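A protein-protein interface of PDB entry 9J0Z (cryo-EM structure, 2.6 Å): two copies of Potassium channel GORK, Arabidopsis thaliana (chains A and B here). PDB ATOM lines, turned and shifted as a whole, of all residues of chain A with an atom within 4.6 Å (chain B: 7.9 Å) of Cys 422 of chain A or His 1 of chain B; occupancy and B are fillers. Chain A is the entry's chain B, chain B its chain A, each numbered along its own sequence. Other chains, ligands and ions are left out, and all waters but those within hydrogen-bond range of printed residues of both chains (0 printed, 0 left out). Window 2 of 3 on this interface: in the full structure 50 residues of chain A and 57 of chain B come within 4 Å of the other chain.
Of the printed residues of chain B, Pro 359 of chain A touches Arg 77 (3.7 Å).
Of chain B, only His 1 (3.5 Å) and Arg 77 (2.6 Å) come within 4 Å of Cys 422 of chain A.
Of the printed residues of chain B, Leu 424 of chain A touches Thr 75 (3.2 Å) and Tyr 76 (3.7 Å).
His 1 of chain B touches just one residue of chain A: Cys 422 (3.5 Å).
Of the printed residues of chain A, Tyr 76 of chain B touches Leu 424.
Tyr 80 of chain B touches none of the printed residues of chain A.
The nearest residue of chain B that does not touch Cys 422 of chain A is Thr 75 of chain B (5.4 Å).
O of Leu 380 of chain A lies within hydrogen-bond range of N of Cys 422 of chain A, 3.1 Å away.
The backbone carbonyl oxygen (O) of Leu 380 of chain A sits at hydrogen-bond distance from the backbone NH (N) of Glu 423 of chain A (2.9 Å).
Printed residues of chain A that touch a printed residue of chain B: Pro 359, Cys 422, Glu 423 and Leu 424.
Hydrophobic or aromatic side chains of chain A within 4 Å of the printed part of chain B: Pro 359 and Leu 424.
Of the 13 printed residues of chain B, 4 touch a printed residue of chain A.
Printed residues of chain B that touch a printed residue of chain A: His 1, Thr 75, Tyr 76 and Arg 77.
Hydrophobic or aromatic side chains of chain B that line the printed part of chain A: His 1 and Tyr 76.
Among the printed residues, Asp or Glu carboxylates within 4 Å of a Lys or Arg side-chain nitrogen of the other chain: Glu 423 of chain A with Arg 77 of chain B (2.5 Å).
No position is printed for both chains.
Pro 359 of chain A touches Arg 77 of chain B (CG to CD, 3.7 Å).
CB of Thr 75 of chain B touches OE1 of Glu 423 of chain A, at 3.3 Å.
Tyr 76 of chain B touches Leu 424 of chain A (CD2 to CD2, 3.7 Å).
A ring nitrogen (NE2) of His 1 of chain B is in hydrogen-bond range of the side-chain sulfur of Cys 422 of chain A (3.5 Å).
O of Thr 75 of chain B sits at hydrogen-bond distance from N of Leu 424 of chain A (3.2 Å).
The guanidinium group of Arg 77 of chain B sits at hydrogen-bond distance from the backbone carbonyl oxygen of Cys 422 of chain A, at 2.6 Å.
NH1 of Arg 77 of chain B lies within salt-bridge range of OE2 of Glu 423 of chain A (2.5 Å).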
ATOM      1  N   PRO A 359      -6.595  25.315  -0.245  1.00  0.00           N
ATOM      2  CA  PRO A 359      -7.286  25.341  -1.544  1.00  0.00           C
ATOM      3  C   PRO A 359      -8.722  24.833  -1.469  1.00  0.00           C
ATOM      4  O   PRO A 359      -9.022  23.859  -0.777  1.00  0.00           O
ATOM      5  CB  PRO A 359      -6.424  24.420  -2.412  1.00  0.00           C
ATOM      6  CG  PRO A 359      -5.078  24.530  -1.840  1.00  0.00           C
ATOM      7  CD  PRO A 359      -5.199  24.865  -0.387  1.00  0.00           C
ATOM      8  N   LEU A 380      -1.012  31.474  -3.652  1.00  0.00           N
ATOM      9  CA  LEU A 380      -1.434  32.110  -4.891  1.00  0.00           C
ATOM     10  C   LEU A 380      -2.888  31.767  -5.171  1.00  0.00           C
ATOM     11  O   LEU A 380      -3.331  30.641  -4.913  1.00  0.00           O
ATOM     12  CB  LEU A 380      -0.523  31.698  -6.057  1.00  0.00           C
ATOM     13  CG  LEU A 380      -0.617  32.448  -7.386  1.00  0.00           C
ATOM     14  CD1 LEU A 380       0.775  32.613  -7.941  1.00  0.00           C
ATOM     15  CD2 LEU A 380      -1.453  31.675  -8.386  1.00  0.00           C
ATOM     16  N   LEU A 381      -3.610  32.745  -5.713  1.00  0.00           N
ATOM     17  CA  LEU A 381      -5.062  32.758  -5.818  1.00  0.00           C
ATOM     18  C   LEU A 381      -5.479  32.516  -7.264  1.00  0.00           C
ATOM     19  O   LEU A 381      -4.656  32.244  -8.137  1.00  0.00           O
ATOM     20  CB  LEU A 381      -5.643  34.086  -5.327  1.00  0.00           C
ATOM     21  CG  LEU A 381      -5.713  34.381  -3.824  1.00  0.00           C
ATOM     22  CD1 LEU A 381      -6.369  33.241  -3.103  1.00  0.00           C
ATOM     23  CD2 LEU A 381      -4.385  34.724  -3.187  1.00  0.00           C
ATOM     24  N   ARG A 420     -10.692  32.446  -6.139  1.00  0.00           N
ATOM     25  CA  ARG A 420     -10.556  31.102  -5.613  1.00  0.00           C
ATOM     26  C   ARG A 420      -9.117  30.894  -5.178  1.00  0.00           C
ATOM     27  O   ARG A 420      -8.203  31.562  -5.672  1.00  0.00           O
ATOM     28  CB  ARG A 420     -10.951  30.067  -6.666  1.00  0.00           C
ATOM     29  CG  ARG A 420     -12.035  29.100  -6.235  1.00  0.00           C
ATOM     30  CD  ARG A 420     -12.329  28.126  -7.354  1.00  0.00           C
ATOM     31  NE  ARG A 420     -11.215  27.197  -7.526  1.00  0.00           N
ATOM     32  CZ  ARG A 420     -11.229  26.148  -8.340  1.00  0.00           C
ATOM     33  NH1 ARG A 420     -12.305  25.884  -9.068  1.00  0.00           N
ATOM     34  NH2 ARG A 420     -10.164  25.363  -8.425  1.00  0.00           N
ATOM     35  N   VAL A 421      -8.921  29.979  -4.248  1.00  0.00           N
ATOM     36  CA  VAL A 421      -7.627  29.795  -3.614  1.00  0.00           C
ATOM     37  C   VAL A 421      -6.973  28.528  -4.155  1.00  0.00           C
ATOM     38  O   VAL A 421      -7.562  27.440  -4.135  1.00  0.00           O
ATOM     39  CB  VAL A 421      -7.777  29.788  -2.080  1.00  0.00           C
ATOM     40  CG1 VAL A 421      -6.458  29.476  -1.393  1.00  0.00           C
ATOM     41  CG2 VAL A 421      -8.342  31.084  -1.586  1.00  0.00           C
ATOM     42  N   CYS A 422      -5.766  28.677  -4.693  1.00  0.00           N
ATOM     43  CA  CYS A 422      -5.103  27.572  -5.370  1.00  0.00           C
ATOM     44  C   CYS A 422      -3.936  27.012  -4.569  1.00  0.00           C
ATOM     45  O   CYS A 422      -3.755  25.798  -4.518  1.00  0.00           O
ATOM     46  CB  CYS A 422      -4.628  28.011  -6.760  1.00  0.00           C
ATOM     47  SG  CYS A 422      -4.270  26.646  -7.882  1.00  0.00           S
ATOM     48  N   GLU A 423      -3.132  27.869  -3.952  1.00  0.00           N
ATOM     49  CA  GLU A 423      -2.050  27.433  -3.081  1.00  0.00           C
ATOM     50  C   GLU A 423      -2.404  27.816  -1.649  1.00  0.00           C
ATOM     51  O   GLU A 423      -3.427  28.451  -1.407  1.00  0.00           O
ATOM     52  CB  GLU A 423      -0.725  28.058  -3.526  1.00  0.00           C
ATOM     53  CG  GLU A 423      -0.340  27.641  -4.946  1.00  0.00           C
ATOM     54  CD  GLU A 423       0.127  26.197  -5.035  1.00  0.00           C
ATOM     55  OE1 GLU A 423       0.873  25.766  -4.144  1.00  0.00           O
ATOM     56  OE2 GLU A 423      -0.271  25.482  -5.975  1.00  0.00           O
ATOM     57  N   LEU A 424      -1.574  27.420  -0.684  1.00  0.00           N
ATOM     58  CA  LEU A 424      -1.919  27.751   0.697  1.00  0.00           C
ATOM     59  C   LEU A 424      -1.636  29.212   0.992  1.00  0.00           C
ATOM     60  O   LEU A 424      -0.472  29.619   1.067  1.00  0.00           O
ATOM     61  CB  LEU A 424      -1.161  26.896   1.704  1.00  0.00           C
ATOM     62  CG  LEU A 424      -1.618  27.287   3.112  1.00  0.00           C
ATOM     63  CD1 LEU A 424      -2.915  26.586   3.436  1.00  0.00           C
ATOM     64  CD2 LEU A 424      -0.556  27.025   4.169  1.00  0.00           C
ATOM     65  N   HIS B   1      -6.122  19.455  -9.112  1.00  0.00           N
ATOM     66  CA  HIS B   1      -5.075  19.497 -10.125  1.00  0.00           C
ATOM     67  C   HIS B   1      -4.730  18.090 -10.589  1.00  0.00           C
ATOM     68  O   HIS B   1      -3.609  17.610 -10.409  1.00  0.00           O
ATOM     69  CB  HIS B   1      -3.834  20.213  -9.586  1.00  0.00           C
ATOM     70  CG  HIS B   1      -3.889  21.699  -9.751  1.00  0.00           C
ATOM     71  ND1 HIS B   1      -2.774  22.462 -10.020  1.00  0.00           N
ATOM     72  CD2 HIS B   1      -4.931  22.562  -9.695  1.00  0.00           C
ATOM     73  CE1 HIS B   1      -3.125  23.732 -10.118  1.00  0.00           C
ATOM     74  NE2 HIS B   1      -4.429  23.819  -9.926  1.00  0.00           N
ATOM     75  N   ASN B   2      -5.721  17.438 -11.197  1.00  0.00           N
ATOM     76  CA  ASN B   2      -5.606  16.050 -11.633  1.00  0.00           C
ATOM     77  C   ASN B   2      -5.265  16.015 -13.121  1.00  0.00           C
ATOM     78  O   ASN B   2      -6.005  15.491 -13.955  1.00  0.00           O
ATOM     79  CB  ASN B   2      -6.898  15.309 -11.332  1.00  0.00           C
ATOM     80  CG  ASN B   2      -7.160  15.184  -9.844  1.00  0.00           C
ATOM     81  OD1 ASN B   2      -8.020  15.870  -9.289  1.00  0.00           O
ATOM     82  ND2 ASN B   2      -6.449  14.272  -9.198  1.00  0.00           N
ATOM     83  N   ASP B   3      -4.108  16.584 -13.457  1.00  0.00           N
ATOM     84  CA  ASP B   3      -3.611  16.578 -14.824  1.00  0.00           C
ATOM     85  C   ASP B   3      -2.656  15.429 -15.086  1.00  0.00           C
ATOM     86  O   ASP B   3      -2.140  15.305 -16.202  1.00  0.00           O
ATOM     87  CB  ASP B   3      -2.913  17.902 -15.149  1.00  0.00           C
ATOM     88  CG  ASP B   3      -1.957  18.342 -14.057  1.00  0.00           C
ATOM     89  OD1 ASP B   3      -2.078  17.838 -12.921  1.00  0.00           O
ATOM     90  OD2 ASP B   3      -1.086  19.192 -14.340  1.00  0.00           O
ATOM     91  N   TYR B   4      -2.410  14.591 -14.089  1.00  0.00           N
ATOM     92  CA  TYR B   4      -1.444  13.510 -14.174  1.00  0.00           C
ATOM     93  C   TYR B   4      -2.166  12.187 -13.986  1.00  0.00           C
ATOM     94  O   TYR B   4      -2.817  11.971 -12.961  1.00  0.00           O
ATOM     95  CB  TYR B   4      -0.357  13.694 -13.127  1.00  0.00           C
ATOM     96  CG  TYR B   4       0.836  14.462 -13.637  1.00  0.00           C
ATOM     97  CD1 TYR B   4       1.804  13.831 -14.403  1.00  0.00           C
ATOM     98  CD2 TYR B   4       0.993  15.819 -13.359  1.00  0.00           C
ATOM     99  CE1 TYR B   4       2.898  14.519 -14.868  1.00  0.00           C
ATOM    100  CE2 TYR B   4       2.092  16.513 -13.810  1.00  0.00           C
ATOM    101  CZ  TYR B   4       3.040  15.855 -14.568  1.00  0.00           C
ATOM    102  OH  TYR B   4       4.139  16.527 -15.044  1.00  0.00           O
ATOM    103  N   HIS B   9      -4.019   8.755  -6.130  1.00  0.00           N
ATOM    104  CA  HIS B   9      -4.398   9.726  -5.130  1.00  0.00           C
ATOM    105  C   HIS B   9      -4.208   9.115  -3.746  1.00  0.00           C
ATOM    106  O   HIS B   9      -4.598   7.970  -3.517  1.00  0.00           O
ATOM    107  CB  HIS B   9      -5.850  10.147  -5.352  1.00  0.00           C
ATOM    108  CG  HIS B   9      -6.198  10.356  -6.797  1.00  0.00           C
ATOM    109  ND1 HIS B   9      -6.481   9.319  -7.659  1.00  0.00           N
ATOM    110  CD2 HIS B   9      -6.298  11.488  -7.530  1.00  0.00           C
ATOM    111  CE1 HIS B   9      -6.733   9.803  -8.860  1.00  0.00           C
ATOM    112  NE2 HIS B   9      -6.632  11.117  -8.808  1.00  0.00           N
ATOM    113  N   ALA B  69       0.954  10.548  -4.907  1.00  0.00           N
ATOM    114  CA  ALA B  69       1.104  11.972  -4.710  1.00  0.00           C
ATOM    115  C   ALA B  69       1.022  12.306  -3.239  1.00  0.00           C
ATOM    116  O   ALA B  69      -0.028  12.180  -2.616  1.00  0.00           O
ATOM    117  CB  ALA B  69       0.017  12.732  -5.452  1.00  0.00           C
ATOM    118  N   THR B  75       2.799  24.304   0.968  1.00  0.00           N
ATOM    119  CA  THR B  75       1.804  24.777   0.025  1.00  0.00           C
ATOM    120  C   THR B  75       0.490  24.040   0.174  1.00  0.00           C
ATOM    121  O   THR B  75      -0.499  24.437  -0.449  1.00  0.00           O
ATOM    122  CB  THR B  75       2.309  24.624  -1.407  1.00  0.00           C
ATOM    123  OG1 THR B  75       2.425  23.236  -1.726  1.00  0.00           O
ATOM    124  CG2 THR B  75       3.662  25.284  -1.555  1.00  0.00           C
ATOM    125  N   TYR B  76       0.481  22.969   0.966  1.00  0.00           N
ATOM    126  CA  TYR B  76      -0.692  22.151   1.280  1.00  0.00           C
ATOM    127  C   TYR B  76      -1.336  21.586   0.022  1.00  0.00           C
ATOM    128  O   TYR B  76      -2.554  21.464  -0.098  1.00  0.00           O
ATOM    129  CB  TYR B  76      -1.683  22.925   2.132  1.00  0.00           C
ATOM    130  CG  TYR B  76      -1.354  22.793   3.586  1.00  0.00           C
ATOM    131  CD1 TYR B  76      -2.165  22.059   4.432  1.00  0.00           C
ATOM    132  CD2 TYR B  76      -0.211  23.379   4.111  1.00  0.00           C
ATOM    133  CE1 TYR B  76      -1.861  21.918   5.765  1.00  0.00           C
ATOM    134  CE2 TYR B  76       0.103  23.251   5.444  1.00  0.00           C
ATOM    135  CZ  TYR B  76      -0.726  22.517   6.267  1.00  0.00           C
ATOM    136  OH  TYR B  76      -0.419  22.379   7.598  1.00  0.00           O
ATOM    137  N   ARG B  77      -0.483  21.223  -0.924  1.00  0.00           N
ATOM    138  CA  ARG B  77      -0.928  20.712  -2.203  1.00  0.00           C
ATOM    139  C   ARG B  77      -0.586  19.240  -2.299  1.00  0.00           C
ATOM    140  O   ARG B  77       0.532  18.831  -1.967  1.00  0.00           O
ATOM    141  CB  ARG B  77      -0.272  21.449  -3.369  1.00  0.00           C
ATOM    142  CG  ARG B  77      -0.489  22.935  -3.383  1.00  0.00           C
ATOM    143  CD  ARG B  77      -1.957  23.278  -3.364  1.00  0.00           C
ATOM    144  NE  ARG B  77      -2.730  22.591  -4.395  1.00  0.00           N
ATOM    145  CZ  ARG B  77      -2.903  23.027  -5.637  1.00  0.00           C
ATOM    146  NH1 ARG B  77      -2.354  24.166  -6.032  1.00  0.00           N
ATOM    147  NH2 ARG B  77      -3.638  22.320  -6.481  1.00  0.00           N
ATOM    148  N   THR B  78      -1.542  18.458  -2.765  1.00  0.00           N
ATOM    149  CA  THR B  78      -1.243  17.114  -3.218  1.00  0.00           C
ATOM    150  C   THR B  78      -0.423  17.251  -4.488  1.00  0.00           C
ATOM    151  O   THR B  78      -0.950  17.569  -5.549  1.00  0.00           O
ATOM    152  CB  THR B  78      -2.533  16.344  -3.450  1.00  0.00           C
ATOM    153  OG1 THR B  78      -3.395  16.515  -2.320  1.00  0.00           O
ATOM    154  N   VAL B  79       0.886  17.051  -4.381  1.00  0.00           N
ATOM    155  CA  VAL B  79       1.774  17.304  -5.508  1.00  0.00           C
ATOM    156  C   VAL B  79       1.675  16.126  -6.462  1.00  0.00           C
ATOM    157  O   VAL B  79       2.399  15.143  -6.310  1.00  0.00           O
ATOM    158  CB  VAL B  79       3.217  17.508  -5.053  1.00  0.00           C
ATOM    159  CG1 VAL B  79       4.047  18.015  -6.200  1.00  0.00           C
ATOM    160  CG2 VAL B  79       3.270  18.460  -3.893  1.00  0.00           C
ATOM    161  N   TYR B  80       0.831  16.230  -7.476  1.00  0.00           N
ATOM    162  CA  TYR B  80       0.566  15.080  -8.336  1.00  0.00           C
ATOM    163  C   TYR B  80       1.645  14.897  -9.380  1.00  0.00           C
ATOM    164  O   TYR B  80       1.310  14.655 -10.516  1.00  0.00           O
ATOM    165  CB  TYR B  80      -0.785  15.245  -9.022  1.00  0.00           C
ATOM    166  CG  TYR B  80      -1.973  14.955  -8.154  1.00  0.00           C
ATOM    167  CD1 TYR B  80      -2.395  13.656  -7.939  1.00  0.00           C
ATOM    168  CD2 TYR B  80      -2.688  15.978  -7.568  1.00  0.00           C
ATOM    169  CE1 TYR B  80      -3.475  13.386  -7.143  1.00  0.00           C
ATOM    170  CE2 TYR B  80      -3.770  15.718  -6.772  1.00  0.00           C
ATOM    171  CZ  TYR B  80      -4.159  14.419  -6.561  1.00  0.00           C
ATOM    172  OH  TYR B  80      -5.243  14.142  -5.772  1.00  0.00           O
ATOM    173  N   LYS B  81       2.930  14.934  -9.054  1.00  0.00           N
ATOM    174  CA  LYS B  81       3.927  15.017 -10.108  1.00  0.00           C
ATOM    175  C   LYS B  81       5.036  14.005  -9.892  1.00  0.00           C
ATOM    176  O   LYS B  81       5.739  14.076  -8.874  1.00  0.00           O
ATOM    177  CB  LYS B  81       4.533  16.412 -10.184  1.00  0.00           C
ATOM    178  CG  LYS B  81       5.695  16.490 -11.148  1.00  0.00           C
ATOM    179  CD  LYS B  81       5.812  17.857 -11.791  1.00  0.00           C
ATOM    180  CE  LYS B  81       6.582  17.791 -13.096  1.00  0.00           C
ATOM    181  NZ  LYS B  81       6.362  19.001 -13.933  1.00  0.00           N
